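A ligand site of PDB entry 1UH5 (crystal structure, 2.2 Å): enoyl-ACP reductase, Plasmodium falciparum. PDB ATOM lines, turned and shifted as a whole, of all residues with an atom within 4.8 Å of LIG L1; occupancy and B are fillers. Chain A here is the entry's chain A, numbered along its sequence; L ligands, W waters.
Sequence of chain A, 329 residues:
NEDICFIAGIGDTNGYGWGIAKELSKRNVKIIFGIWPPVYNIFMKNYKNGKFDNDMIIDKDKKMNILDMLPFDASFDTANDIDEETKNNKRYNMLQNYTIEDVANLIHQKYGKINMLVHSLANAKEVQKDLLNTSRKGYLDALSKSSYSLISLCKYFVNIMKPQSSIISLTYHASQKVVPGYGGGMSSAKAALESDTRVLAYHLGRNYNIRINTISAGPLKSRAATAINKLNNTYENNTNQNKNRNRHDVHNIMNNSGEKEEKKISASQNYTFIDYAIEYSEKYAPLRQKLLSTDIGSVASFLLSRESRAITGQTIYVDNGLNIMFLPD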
ATOM      1  N   GLY A   9       8.771  29.992   5.803  1.00  0.00           N
ATOM      2  CA  GLY A   9       9.336  29.891   4.461  1.00  0.00           C
ATOM      3  C   GLY A   9       8.472  30.441   3.342  1.00  0.00           C
ATOM      4  O   GLY A   9       8.001  29.692   2.490  1.00  0.00           O
ATOM      5  N   ILE A  10       8.278  31.753   3.332  1.00  0.00           N
ATOM      6  CA  ILE A  10       7.490  32.406   2.297  1.00  0.00           C
ATOM      7  C   ILE A  10       8.181  33.695   1.866  1.00  0.00           C
ATOM      8  O   ILE A  10       8.517  34.534   2.701  1.00  0.00           O
ATOM      9  CB  ILE A  10       6.068  32.753   2.792  1.00  0.00           C
ATOM     10  CG1 ILE A  10       5.267  31.463   2.988  1.00  0.00           C
ATOM     11  CG2 ILE A  10       5.371  33.674   1.795  1.00  0.00           C
ATOM     12  CD1 ILE A  10       3.822  31.702   3.381  1.00  0.00           C
ATOM     13  N   GLY A  11       8.407  33.837   0.564  1.00  0.00           N
ATOM     14  CA  GLY A  11       9.065  35.026   0.051  1.00  0.00           C
ATOM     15  C   GLY A  11       8.262  35.707  -1.039  1.00  0.00           C
ATOM     16  O   GLY A  11       8.595  36.806  -1.495  1.00  0.00           O
ATOM     17  N   ASP A  12       7.196  35.035  -1.470  1.00  0.00           N
ATOM     18  CA  ASP A  12       6.328  35.542  -2.513  1.00  0.00           C
ATOM     19  C   ASP A  12       5.076  34.670  -2.571  1.00  0.00           C
ATOM     20  O   ASP A  12       4.822  33.898  -1.644  1.00  0.00           O
ATOM     21  CB  ASP A  12       7.038  35.503  -3.866  1.00  0.00           C
ATOM     22  CG  ASP A  12       7.513  34.110  -4.218  1.00  0.00           C
ATOM     23  OD1 ASP A  12       8.477  33.643  -3.568  1.00  0.00           O
ATOM     24  OD2 ASP A  12       6.933  33.484  -5.117  1.00  0.00           O
ATOM     25  N   GLY A  15       5.266  30.136  -4.584  1.00  0.00           N
ATOM     26  CA  GLY A  15       5.719  28.866  -4.051  1.00  0.00           C
ATOM     27  C   GLY A  15       4.622  28.052  -3.394  1.00  0.00           C
ATOM     28  O   GLY A  15       3.449  28.414  -3.443  1.00  0.00           O
ATOM     29  N   TYR A  16       5.009  26.938  -2.787  1.00  0.00           N
ATOM     30  CA  TYR A  16       4.062  26.050  -2.113  1.00  0.00           C
ATOM     31  C   TYR A  16       3.559  26.621  -0.797  1.00  0.00           C
ATOM     32  O   TYR A  16       2.460  26.293  -0.353  1.00  0.00           O
ATOM     33  CB  TYR A  16       4.707  24.682  -1.872  1.00  0.00           C
ATOM     34  CG  TYR A  16       4.671  23.777  -3.090  1.00  0.00           C
ATOM     35  CD1 TYR A  16       3.470  23.483  -3.724  1.00  0.00           C
ATOM     36  CD2 TYR A  16       5.837  23.204  -3.590  1.00  0.00           C
ATOM     37  CE1 TYR A  16       3.418  22.648  -4.838  1.00  0.00           C
ATOM     38  CE2 TYR A  16       5.807  22.361  -4.704  1.00  0.00           C
ATOM     39  CZ  TYR A  16       4.597  22.093  -5.315  1.00  0.00           C
ATOM     40  OH  TYR A  16       4.554  21.256  -6.418  1.00  0.00           O
ATOM     41  N   GLY A  17       4.358  27.466  -0.162  1.00  0.00           N
ATOM     42  CA  GLY A  17       3.948  28.076   1.096  1.00  0.00           C
ATOM     43  C   GLY A  17       2.666  28.861   0.906  1.00  0.00           C
ATOM     44  O   GLY A  17       1.731  28.771   1.713  1.00  0.00           O
ATOM     45  N   TRP A  36      12.027  35.120   5.530  1.00  0.00           N
ATOM     46  CA  TRP A  36      13.478  35.222   5.559  1.00  0.00           C
ATOM     47  C   TRP A  36      13.850  36.710   5.531  1.00  0.00           C
ATOM     48  O   TRP A  36      13.512  37.432   4.592  1.00  0.00           O
ATOM     49  CB  TRP A  36      14.046  34.480   4.343  1.00  0.00           C
ATOM     50  CG  TRP A  36      15.531  34.287   4.357  1.00  0.00           C
ATOM     51  CD1 TRP A  36      16.320  34.049   5.447  1.00  0.00           C
ATOM     52  CD2 TRP A  36      16.406  34.272   3.219  1.00  0.00           C
ATOM     53  NE1 TRP A  36      17.619  33.880   5.060  1.00  0.00           N
ATOM     54  CE2 TRP A  36      17.705  34.009   3.701  1.00  0.00           C
ATOM     55  CE3 TRP A  36      16.206  34.450   1.846  1.00  0.00           C
ATOM     56  CZ2 TRP A  36      18.810  33.924   2.842  1.00  0.00           C
ATOM     57  CZ3 TRP A  36      17.311  34.352   0.993  1.00  0.00           C
ATOM     58  CH2 TRP A  36      18.594  34.096   1.508  1.00  0.00           C
ATOM     59  N   VAL A  39      14.629  39.185   2.495  1.00  0.00           N
ATOM     60  CA  VAL A  39      13.559  39.623   1.600  1.00  0.00           C
ATOM     61  C   VAL A  39      12.309  40.064   2.378  1.00  0.00           C
ATOM     62  O   VAL A  39      11.232  40.196   1.803  1.00  0.00           O
ATOM     63  CB  VAL A  39      13.142  38.498   0.621  1.00  0.00           C
ATOM     64  CG1 VAL A  39      14.371  37.912  -0.064  1.00  0.00           C
ATOM     65  CG2 VAL A  39      12.365  37.417   1.341  1.00  0.00           C
ATOM     66  N   PHE A  72      12.045  35.707   9.956  1.00  0.00           N
ATOM     67  CA  PHE A  72      12.399  34.412  10.508  1.00  0.00           C
ATOM     68  C   PHE A  72      13.573  33.808   9.752  1.00  0.00           C
ATOM     69  O   PHE A  72      13.518  33.676   8.528  1.00  0.00           O
ATOM     70  CB  PHE A  72      11.179  33.483  10.392  1.00  0.00           C
ATOM     71  CG  PHE A  72      11.435  32.056  10.777  1.00  0.00           C
ATOM     72  CD1 PHE A  72      11.408  31.657  12.104  1.00  0.00           C
ATOM     73  CD2 PHE A  72      11.679  31.096   9.800  1.00  0.00           C
ATOM     74  CE1 PHE A  72      11.613  30.316  12.459  1.00  0.00           C
ATOM     75  CE2 PHE A  72      11.895  29.759  10.129  1.00  0.00           C
ATOM     76  CZ  PHE A  72      11.856  29.365  11.468  1.00  0.00           C
ATOM     77  N   ASP A  73      14.634  33.475  10.467  1.00  0.00           N
ATOM     78  CA  ASP A  73      15.790  32.869   9.828  1.00  0.00           C
ATOM     79  C   ASP A  73      16.064  31.516  10.477  1.00  0.00           C
ATOM     80  O   ASP A  73      16.444  31.443  11.646  1.00  0.00           O
ATOM     81  CB  ASP A  73      17.024  33.754   9.950  1.00  0.00           C
ATOM     82  CG  ASP A  73      18.118  33.352   8.994  1.00  0.00           C
ATOM     83  OD1 ASP A  73      18.321  32.132   8.814  1.00  0.00           O
ATOM     84  OD2 ASP A  73      18.786  34.240   8.417  1.00  0.00           O
ATOM     85  N   ALA A  74      15.864  30.453   9.708  1.00  0.00           N
ATOM     86  CA  ALA A  74      16.059  29.090  10.187  1.00  0.00           C
ATOM     87  C   ALA A  74      17.517  28.714  10.446  1.00  0.00           C
ATOM     88  O   ALA A  74      17.799  27.610  10.890  1.00  0.00           O
ATOM     89  CB  ALA A  74      15.425  28.103   9.196  1.00  0.00           C
ATOM     90  N   SER A  75      18.434  29.630  10.156  1.00  0.00           N
ATOM     91  CA  SER A  75      19.854  29.390  10.359  1.00  0.00           C
ATOM     92  C   SER A  75      20.245  29.556  11.829  1.00  0.00           C
ATOM     93  O   SER A  75      21.252  29.010  12.283  1.00  0.00           O
ATOM     94  CB  SER A  75      20.684  30.402   9.550  1.00  0.00           C
ATOM     95  OG  SER A  75      20.364  30.362   8.165  1.00  0.00           O
ATOM     96  N   SER A 120       8.358  24.947   5.141  1.00  0.00           N
ATOM     97  CA  SER A 120       8.390  25.022   3.683  1.00  0.00           C
ATOM     98  C   SER A 120       9.600  25.813   3.206  1.00  0.00           C
ATOM     99  O   SER A 120       9.469  26.773   2.454  1.00  0.00           O
ATOM    100  CB  SER A 120       7.111  25.692   3.155  1.00  0.00           C
ATOM    101  OG  SER A 120       7.105  25.739   1.740  1.00  0.00           O
ATOM    102  N   LEU A 121      10.777  25.397   3.648  1.00  0.00           N
ATOM    103  CA  LEU A 121      11.990  26.095   3.257  1.00  0.00           C
ATOM    104  C   LEU A 121      13.139  25.151   2.986  1.00  0.00           C
ATOM    105  O   LEU A 121      13.217  24.054   3.543  1.00  0.00           O
ATOM    106  CB  LEU A 121      12.382  27.102   4.340  1.00  0.00           C
ATOM    107  CG  LEU A 121      12.632  26.543   5.745  1.00  0.00           C
ATOM    108  CD1 LEU A 121      14.066  26.069   5.841  1.00  0.00           C
ATOM    109  CD2 LEU A 121      12.353  27.613   6.778  1.00  0.00           C
ATOM    110  N   ALA A 122      14.012  25.580   2.091  1.00  0.00           N
ATOM    111  CA  ALA A 122      15.188  24.813   1.711  1.00  0.00           C
ATOM    112  C   ALA A 122      16.195  25.821   1.194  1.00  0.00           C
ATOM    113  O   ALA A 122      15.824  26.867   0.660  1.00  0.00           O
ATOM    114  CB  ALA A 122      14.838  23.816   0.616  1.00  0.00           C
ATOM    115  N   ASN A 123      17.477  25.517   1.364  1.00  0.00           N
ATOM    116  CA  ASN A 123      18.516  26.412   0.904  1.00  0.00           C
ATOM    117  C   ASN A 123      19.827  25.645   0.823  1.00  0.00           C
ATOM    118  O   ASN A 123      20.145  24.841   1.703  1.00  0.00           O
ATOM    119  CB  ASN A 123      18.646  27.599   1.864  1.00  0.00           C
ATOM    120  CG  ASN A 123      19.245  28.832   1.196  1.00  0.00           C
ATOM    121  OD1 ASN A 123      19.266  29.907   1.781  1.00  0.00           O
ATOM    122  ND2 ASN A 123      19.733  28.664  -0.034  1.00  0.00           N
ATOM    123  N   LYS A 145      20.293  24.324   6.959  1.00  0.00           N
ATOM    124  CA  LYS A 145      19.123  25.138   6.657  1.00  0.00           C
ATOM    125  C   LYS A 145      17.911  24.367   6.154  1.00  0.00           C
ATOM    126  O   LYS A 145      16.778  24.783   6.375  1.00  0.00           O
ATOM    127  CB  LYS A 145      19.510  26.224   5.661  1.00  0.00           C
ATOM    128  CG  LYS A 145      20.542  27.179   6.236  1.00  0.00           C
ATOM    129  CD  LYS A 145      21.168  28.021   5.152  1.00  0.00           C
ATOM    130  CE  LYS A 145      22.190  29.002   5.750  1.00  0.00           C
ATOM    131  NZ  LYS A 145      22.934  29.667   4.647  1.00  0.00           N
ATOM    132  N   LEU A 170       8.019  19.811   3.336  1.00  0.00           N
ATOM    133  CA  LEU A 170       7.980  19.441   1.928  1.00  0.00           C
ATOM    134  C   LEU A 170       9.301  18.791   1.524  1.00  0.00           C
ATOM    135  O   LEU A 170      10.378  19.245   1.918  1.00  0.00           O
ATOM    136  CB  LEU A 170       7.717  20.678   1.073  1.00  0.00           C
ATOM    137  CG  LEU A 170       6.346  21.334   1.306  1.00  0.00           C
ATOM    138  CD1 LEU A 170       6.341  22.743   0.748  1.00  0.00           C
ATOM    139  CD2 LEU A 170       5.263  20.494   0.643  1.00  0.00           C
ATOM    140  N   THR A 171       9.214  17.727   0.745  1.00  0.00           N
ATOM    141  CA  THR A 171      10.418  17.043   0.289  1.00  0.00           C
ATOM    142  C   THR A 171      10.320  16.794  -1.208  1.00  0.00           C
ATOM    143  O   THR A 171       9.376  17.253  -1.857  1.00  0.00           O
ATOM    144  CB  THR A 171      10.619  15.703   1.058  1.00  0.00           C
ATOM    145  OG1 THR A 171      11.898  15.144   0.720  1.00  0.00           O
ATOM    146  CG2 THR A 171       9.502  14.706   0.719  1.00  0.00           C
ATOM    147  N   TYR A 172      11.284  16.069  -1.757  1.00  0.00           N
ATOM    148  CA  TYR A 172      11.289  15.799  -3.185  1.00  0.00           C
ATOM    149  C   TYR A 172      11.899  14.420  -3.413  1.00  0.00           C
ATOM    150  O   TYR A 172      12.812  14.005  -2.699  1.00  0.00           O
ATOM    151  CB  TYR A 172      12.086  16.899  -3.918  1.00  0.00           C
ATOM    152  CG  TYR A 172      12.128  16.764  -5.426  1.00  0.00           C
ATOM    153  CD1 TYR A 172      10.954  16.634  -6.164  1.00  0.00           C
ATOM    154  CD2 TYR A 172      13.344  16.755  -6.106  1.00  0.00           C
ATOM    155  CE1 TYR A 172      10.986  16.491  -7.555  1.00  0.00           C
ATOM    156  CE2 TYR A 172      13.389  16.624  -7.505  1.00  0.00           C
ATOM    157  CZ  TYR A 172      12.205  16.490  -8.217  1.00  0.00           C
ATOM    158  OH  TYR A 172      12.247  16.335  -9.582  1.00  0.00           O
ATOM    159  N   TYR A 182      19.789  18.127  -9.331  1.00  0.00           N
ATOM    160  CA  TYR A 182      19.450  18.449  -7.942  1.00  0.00           C
ATOM    161  C   TYR A 182      20.695  18.304  -7.080  1.00  0.00           C
ATOM    162  O   TYR A 182      20.819  17.361  -6.290  1.00  0.00           O
ATOM    163  CB  TYR A 182      18.353  17.484  -7.462  1.00  0.00           C
ATOM    164  CG  TYR A 182      17.519  17.988  -6.311  1.00  0.00           C
ATOM    165  CD1 TYR A 182      16.682  19.090  -6.461  1.00  0.00           C
ATOM    166  CD2 TYR A 182      17.565  17.347  -5.076  1.00  0.00           C
ATOM    167  CE1 TYR A 182      15.901  19.537  -5.405  1.00  0.00           C
ATOM    168  CE2 TYR A 182      16.784  17.782  -4.014  1.00  0.00           C
ATOM    169  CZ  TYR A 182      15.944  18.874  -4.182  1.00  0.00           C
ATOM    170  OH  TYR A 182      15.154  19.281  -3.128  1.00  0.00           O
ATOM    171  N   MET A 186      21.298  18.916  -1.758  1.00  0.00           N
ATOM    172  CA  MET A 186      19.862  19.044  -1.539  1.00  0.00           C
ATOM    173  C   MET A 186      19.216  17.666  -1.511  1.00  0.00           C
ATOM    174  O   MET A 186      18.237  17.444  -0.803  1.00  0.00           O
ATOM    175  CB  MET A 186      19.203  19.890  -2.632  1.00  0.00           C
ATOM    176  CG  MET A 186      19.261  21.382  -2.346  1.00  0.00           C
ATOM    177  SD  MET A 186      18.592  21.774  -0.717  1.00  0.00           S
ATOM    178  CE  MET A 186      16.938  21.124  -0.847  1.00  0.00           C
ATOM    179  N   LYS A 190      17.201  16.217   1.674  1.00  0.00           N
ATOM    180  CA  LYS A 190      15.842  15.698   1.596  1.00  0.00           C
ATOM    181  C   LYS A 190      15.785  14.263   2.132  1.00  0.00           C
ATOM    182  O   LYS A 190      14.784  13.853   2.719  1.00  0.00           O
ATOM    183  CB  LYS A 190      15.310  15.749   0.164  1.00  0.00           C
ATOM    184  CG  LYS A 190      15.033  17.165  -0.346  1.00  0.00           C
ATOM    185  CD  LYS A 190      14.092  17.929   0.594  1.00  0.00           C
ATOM    186  CE  LYS A 190      13.715  19.295   0.013  1.00  0.00           C
ATOM    187  NZ  LYS A 190      12.898  20.131   0.953  1.00  0.00           N
ATOM    188  N   ALA A 217       6.353  16.728  -3.041  1.00  0.00           N
ATOM    189  CA  ALA A 217       5.666  17.416  -4.122  1.00  0.00           C
ATOM    190  C   ALA A 217       6.333  17.282  -5.491  1.00  0.00           C
ATOM    191  O   ALA A 217       7.523  17.029  -5.596  1.00  0.00           O
ATOM    192  CB  ALA A 217       5.525  18.894  -3.771  1.00  0.00           C
ATOM    193  N   GLY A 218       5.521  17.466  -6.530  1.00  0.00           N
ATOM    194  CA  GLY A 218       6.013  17.429  -7.899  1.00  0.00           C
ATOM    195  C   GLY A 218       6.570  18.790  -8.249  1.00  0.00           C
ATOM    196  O   GLY A 218       6.501  19.717  -7.423  1.00  0.00           O
ATOM    197  N   PRO A 219       7.107  18.974  -9.460  1.00  0.00           N
ATOM    198  CA  PRO A 219       7.674  20.273  -9.862  1.00  0.00           C
ATOM    199  C   PRO A 219       6.683  21.418  -9.959  1.00  0.00           C
ATOM    200  O   PRO A 219       5.552  21.271 -10.429  1.00  0.00           O
ATOM    201  CB  PRO A 219       8.347  19.966 -11.185  1.00  0.00           C
ATOM    202  CG  PRO A 219       7.438  18.916 -11.772  1.00  0.00           C
ATOM    203  CD  PRO A 219       7.149  18.015 -10.579  1.00  0.00           C
ATOM    204  N   LEU A 220       7.133  22.587  -9.497  1.00  0.00           N
ATOM    205  CA  LEU A 220       6.360  23.819  -9.518  1.00  0.00           C
ATOM    206  C   LEU A 220       7.349  24.938  -9.826  1.00  0.00           C
ATOM    207  O   LEU A 220       8.341  25.106  -9.116  1.00  0.00           O
ATOM    208  CB  LEU A 220       5.704  24.052  -8.153  1.00  0.00           C
ATOM    209  CG  LEU A 220       4.954  25.375  -7.974  1.00  0.00           C
ATOM    210  CD1 LEU A 220       3.783  25.412  -8.923  1.00  0.00           C
ATOM    211  CD2 LEU A 220       4.485  25.515  -6.533  1.00  0.00           C
ATOM    212  N   SER A 222       8.647  27.812  -9.179  1.00  0.00           N
ATOM    213  CA  SER A 222       8.682  28.819  -8.130  1.00  0.00           C
ATOM    214  C   SER A 222       9.948  29.649  -8.234  1.00  0.00           C
ATOM    215  O   SER A 222      10.710  29.516  -9.196  1.00  0.00           O
ATOM    216  CB  SER A 222       8.635  28.148  -6.752  1.00  0.00           C
ATOM    217  OG  SER A 222       9.823  27.389  -6.535  1.00  0.00           O
ATOM    218  N   ARG A 223      10.181  30.496  -7.238  1.00  0.00           N
ATOM    219  CA  ARG A 223      11.358  31.349  -7.235  1.00  0.00           C
ATOM    220  C   ARG A 223      12.651  30.568  -7.072  1.00  0.00           C
ATOM    221  O   ARG A 223      13.574  30.718  -7.882  1.00  0.00           O
ATOM    222  N   ALA A 224      12.721  29.737  -6.033  1.00  0.00           N
ATOM    223  CA  ALA A 224      13.921  28.945  -5.769  1.00  0.00           C
ATOM    224  C   ALA A 224      14.193  27.910  -6.862  1.00  0.00           C
ATOM    225  O   ALA A 224      15.344  27.644  -7.199  1.00  0.00           O
ATOM    226  CB  ALA A 224      13.797  28.257  -4.425  1.00  0.00           C
ATOM    227  N   ALA A 225      13.122  27.335  -7.403  1.00  0.00           N
ATOM    228  CA  ALA A 225      13.253  26.326  -8.448  1.00  0.00           C
ATOM    229  C   ALA A 225      14.062  26.848  -9.631  1.00  0.00           C
ATOM    230  O   ALA A 225      14.897  26.134 -10.183  1.00  0.00           O
ATOM    231  CB  ALA A 225      11.869  25.895  -8.930  1.00  0.00           C
HETATM  232  P1  LIG L   1      10.272  29.300  -2.430  1.00  0.00           P
HETATM  233  O1  LIG L   1      11.681  29.350  -2.871  1.00  0.00           O
HETATM  234  O2  LIG L   1       9.002  29.194  -3.194  1.00  0.00           O
HETATM  235  O3  LIG L   1      10.182  28.750  -0.921  1.00  0.00           O
HETATM  236  C1  LIG L   1      11.364  28.535  -0.071  1.00  0.00           C
HETATM  237  C2  LIG L   1      11.384  29.650   0.942  1.00  0.00           C
HETATM  238  O4  LIG L   1      12.556  29.419   1.824  1.00  0.00           O
HETATM  239  C3  LIG L   1      11.616  31.100   0.377  1.00  0.00           C
HETATM  240  O5  LIG L   1      10.459  31.952   0.670  1.00  0.00           O
HETATM  241  C4  LIG L   1      12.909  31.584   1.031  1.00  0.00           C
HETATM  242  O6  LIG L   1      13.055  32.941   1.239  1.00  0.00           O
HETATM  243  C5  LIG L   1      12.911  30.708   2.282  1.00  0.00           C
HETATM  244  N1  LIG L   1      14.226  30.589   2.907  1.00  0.00           N
HETATM  245  C6  LIG L   1      15.508  30.355   2.396  1.00  0.00           C
HETATM  246  N2  LIG L   1      16.449  30.325   3.340  1.00  0.00           N
HETATM  247  C7  LIG L   1      15.849  30.553   4.519  1.00  0.00           C
HETATM  248  C8  LIG L   1      16.330  30.644   5.906  1.00  0.00           C
HETATM  249  N3  LIG L   1      17.614  30.497   6.215  1.00  0.00           N
HETATM  250  N4  LIG L   1      15.351  30.901   6.862  1.00  0.00           N
HETATM  251  C9  LIG L   1      14.042  31.052   6.613  1.00  0.00           C
HETATM  252  N5  LIG L   1      13.510  30.974   5.308  1.00  0.00           N
HETATM  253  C10 LIG L   1      14.450  30.719   4.290  1.00  0.00           C
HETATM  254  O7  LIG L   1      10.393  27.725  -2.788  1.00  0.00           O
HETATM  255  P2  LIG L   1       9.356  26.475  -3.125  1.00  0.00           P
HETATM  256  O8  LIG L   1       9.666  26.001  -4.472  1.00  0.00           O
HETATM  257  O9  LIG L   1       7.966  26.935  -2.777  1.00  0.00           O
HETATM  258  O10 LIG L   1       9.868  25.352  -2.102  1.00  0.00           O
HETATM  259  C11 LIG L   1       9.678  25.489  -0.667  1.00  0.00           C
HETATM  260  C12 LIG L   1       9.812  24.158  -0.046  1.00  0.00           C
HETATM  261  O11 LIG L   1       9.034  23.168  -0.864  1.00  0.00           O
HETATM  262  C13 LIG L   1      11.258  23.566  -0.054  1.00  0.00           C
HETATM  263  O12 LIG L   1      11.442  22.727   1.113  1.00  0.00           O
HETATM  264  C14 LIG L   1      11.313  22.747  -1.362  1.00  0.00           C
HETATM  265  O13 LIG L   1      12.402  21.871  -1.362  1.00  0.00           O
HETATM  266  C15 LIG L   1       9.895  22.081  -1.317  1.00  0.00           C
HETATM  267  N6  LIG L   1       9.234  21.556  -2.571  1.00  0.00           N
HETATM  268  C16 LIG L   1       9.218  22.364  -3.799  1.00  0.00           C
HETATM  269  C17 LIG L   1       9.253  21.848  -5.053  1.00  0.00           C
HETATM  270  C18 LIG L   1       9.190  22.751  -6.294  1.00  0.00           C
HETATM  271  O14 LIG L   1       8.920  22.220  -7.394  1.00  0.00           O
HETATM  272  N7  LIG L   1       9.418  24.079  -6.188  1.00  0.00           N
HETATM  273  C19 LIG L   1       9.364  20.333  -5.314  1.00  0.00           C
HETATM  274  C20 LIG L   1       9.456  19.512  -4.050  1.00  0.00           C
HETATM  275  C21 LIG L   1       9.395  20.125  -2.769  1.00  0.00           C
HETATM  276  C1  LG2 L   2      12.714  20.497  -5.845  1.00  0.00           C
HETATM  277  C2  LG2 L   2      12.454  21.059  -7.138  1.00  0.00           C
HETATM  278  C3  LG2 L   2      13.017  21.361  -4.781  1.00  0.00           C
HETATM  279  C4  LG2 L   2      13.068  22.812  -5.011  1.00  0.00           C
HETATM  280  C5  LG2 L   2      12.797  23.348  -6.312  1.00  0.00           C
HETATM  281  C6  LG2 L   2      12.492  22.492  -7.391  1.00  0.00           C
HETATM  282  C7  LG2 L   2      17.287  25.343  -3.053  1.00  0.00           C
HETATM  283  C8  LG2 L   2      16.088  25.852  -2.383  1.00  0.00           C
HETATM  284  C9  LG2 L   2      14.817  25.276  -2.697  1.00  0.00           C
HETATM  285  C10 LG2 L   2      14.702  24.174  -3.676  1.00  0.00           C
HETATM  286  C11 LG2 L   2      17.200  24.276  -4.008  1.00  0.00           C
HETATM  287  C12 LG2 L   2      15.910  23.698  -4.306  1.00  0.00           C
HETATM  288  O1  LG2 L   2      13.378  23.645  -3.934  1.00  0.00           O
HETATM  289 CL1  LG2 L   2      12.058  19.975  -8.441  1.00  0.00          CL
HETATM  290 CL2  LG2 L   2      18.814  26.021  -2.700  1.00  0.00          CL
HETATM  291 CL3  LG2 L   2      13.407  25.932  -1.865  1.00  0.00          CL
HETATM  292  O2  LG2 L   2      13.268  20.868  -3.574  1.00  0.00           O
HETATM  293  O   HOH W   1      10.424  21.775   3.615  1.00  0.00           O
HETATM  294  O   HOH W   2       8.046  32.030  -1.440  1.00  0.00           O
HETATM  295  O   HOH W   3      13.771  21.245   3.147  1.00  0.00           O
HETATM  296  O   HOH W   4      10.753  33.711   3.032  1.00  0.00           O
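O of Leu 220 lies within hydrogen-bond range of N7 of LIG L1 (3.3 Å).
The side-chain carboxylate (OD1) of Asp 73 sits at hydrogen-bond distance from a nitrogen (N3) of LIG L1, at 3.2 Å.
The backbone NH of Gly 11 sits at hydrogen-bond distance from an oxygen (O5) of LIG L1, 2.8 Å away.
O2 of LG2 L2 lies within hydrogen-bond range of OH of Tyr 182 (2.5 Å).
The side-chain hydroxyl (OG) of Ser 222 is in hydrogen-bond range of an oxygen (O8) of LIG L1.
O14 of LIG L1 lies within hydrogen-bond range of N of Leu 220 (2.8 Å).
NZ of Lys 190 sits at hydrogen-bond distance from O13 of LIG L1, 2.9 Å away.
The backbone NH (N) of Ile 10 sits close to an oxygen (O5) of LIG L1 (3.4 Å).
The backbone NH (N) of Tyr 16 lies within hydrogen-bond range of an oxygen (O9) of LIG L1 (3.0 Å).
O of Leu 121 sits at hydrogen-bond distance from O12 of LIG L1 (3.3 Å).
OG of Ser 75 is in hydrogen-bond range of N3 of LIG L1 (3.4 Å).
A nitrogen (N2) of LIG L1 sits close to the side-chain amide oxygen (OD1) of Asn 123 (3.2 Å).
A nitrogen (N4) of LIG L1 sits at hydrogen-bond distance from the backbone NH (N) of Ala 74 (2.9 Å).
N of Ala 224 lies close to O1 of LIG L1, 3.4 Å away.
An oxygen (O13) of LIG L1 is in hydrogen-bond range of an oxygen (O2) of LG2 L2 (2.6 Å).
Water W1 lies within hydrogen-bond range of an oxygen (O12) of LIG L1 (2.9 Å) and the backbone carbonyl oxygen of Leu 170 (3.0 Å).
Water W4 lies within hydrogen-bond range of the backbone carbonyl oxygen (O) of Ile 10 (2.4 Å), an oxygen (O5) of LIG L1 (3.0 Å), the backbone NH (N) of Trp 36 (3.1 Å) and the backbone NH (N) of Gly 11 (3.4 Å).
Water W2 lies within hydrogen-bond range of the side-chain carboxylate of Asp 12 (2.7 Å), the backbone NH of Gly 11 (2.7 Å) and an oxygen (O5) of LIG L1 (3.2 Å).
Water W3 lies within hydrogen-bond range of the side-chain amino group (NZ) of Lys 190 (2.6 Å), the backbone carbonyl oxygen (O) of Leu 121 (2.9 Å) and an oxygen (O12) of LIG L1 (3.4 Å).
O of Thr 171 lies within hydrogen-bond range of N of Ala 217.
The backbone carbonyl oxygen (O) of Gly 218 lies within hydrogen-bond range of the side-chain hydroxyl (OH) of Tyr 16 (2.7 Å).
OG of Ser 222 is in hydrogen-bond range of N of Ala 225 (3.4 Å).
The side-chain carboxylate of Asp 73 sits at hydrogen-bond distance from the side-chain hydroxyl of Ser 75, 2.8 Å away.
O of Leu 170 lies within hydrogen-bond range of NZ of Lys 190, 2.8 Å away.
O14 of LIG L1 sits close to O of Gly 218 (3.5 Å).
Merely in contact with LIG L1: Gly 9 (3.7 Å), Gly 15 (3.2 Å), Trp 36 (3.4 Å), Phe 72 (3.3 Å), Ser 120 (3.4 Å), Ala 122 (3.6 Å), Leu 170 (3.2 Å), Thr 171 (3.0 Å), Tyr 172 (3.7 Å), Ala 217 (3.5 Å) and Pro 219 (3.4 Å).
Hydrophobic or aromatic side chains within 4 Å of LIG L1: Tyr 16, Trp 36, Phe 72, Ala 74, Leu 121, Ala 122, Leu 170, Tyr 172, Ala 217, Leu 220 and Ala 224.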
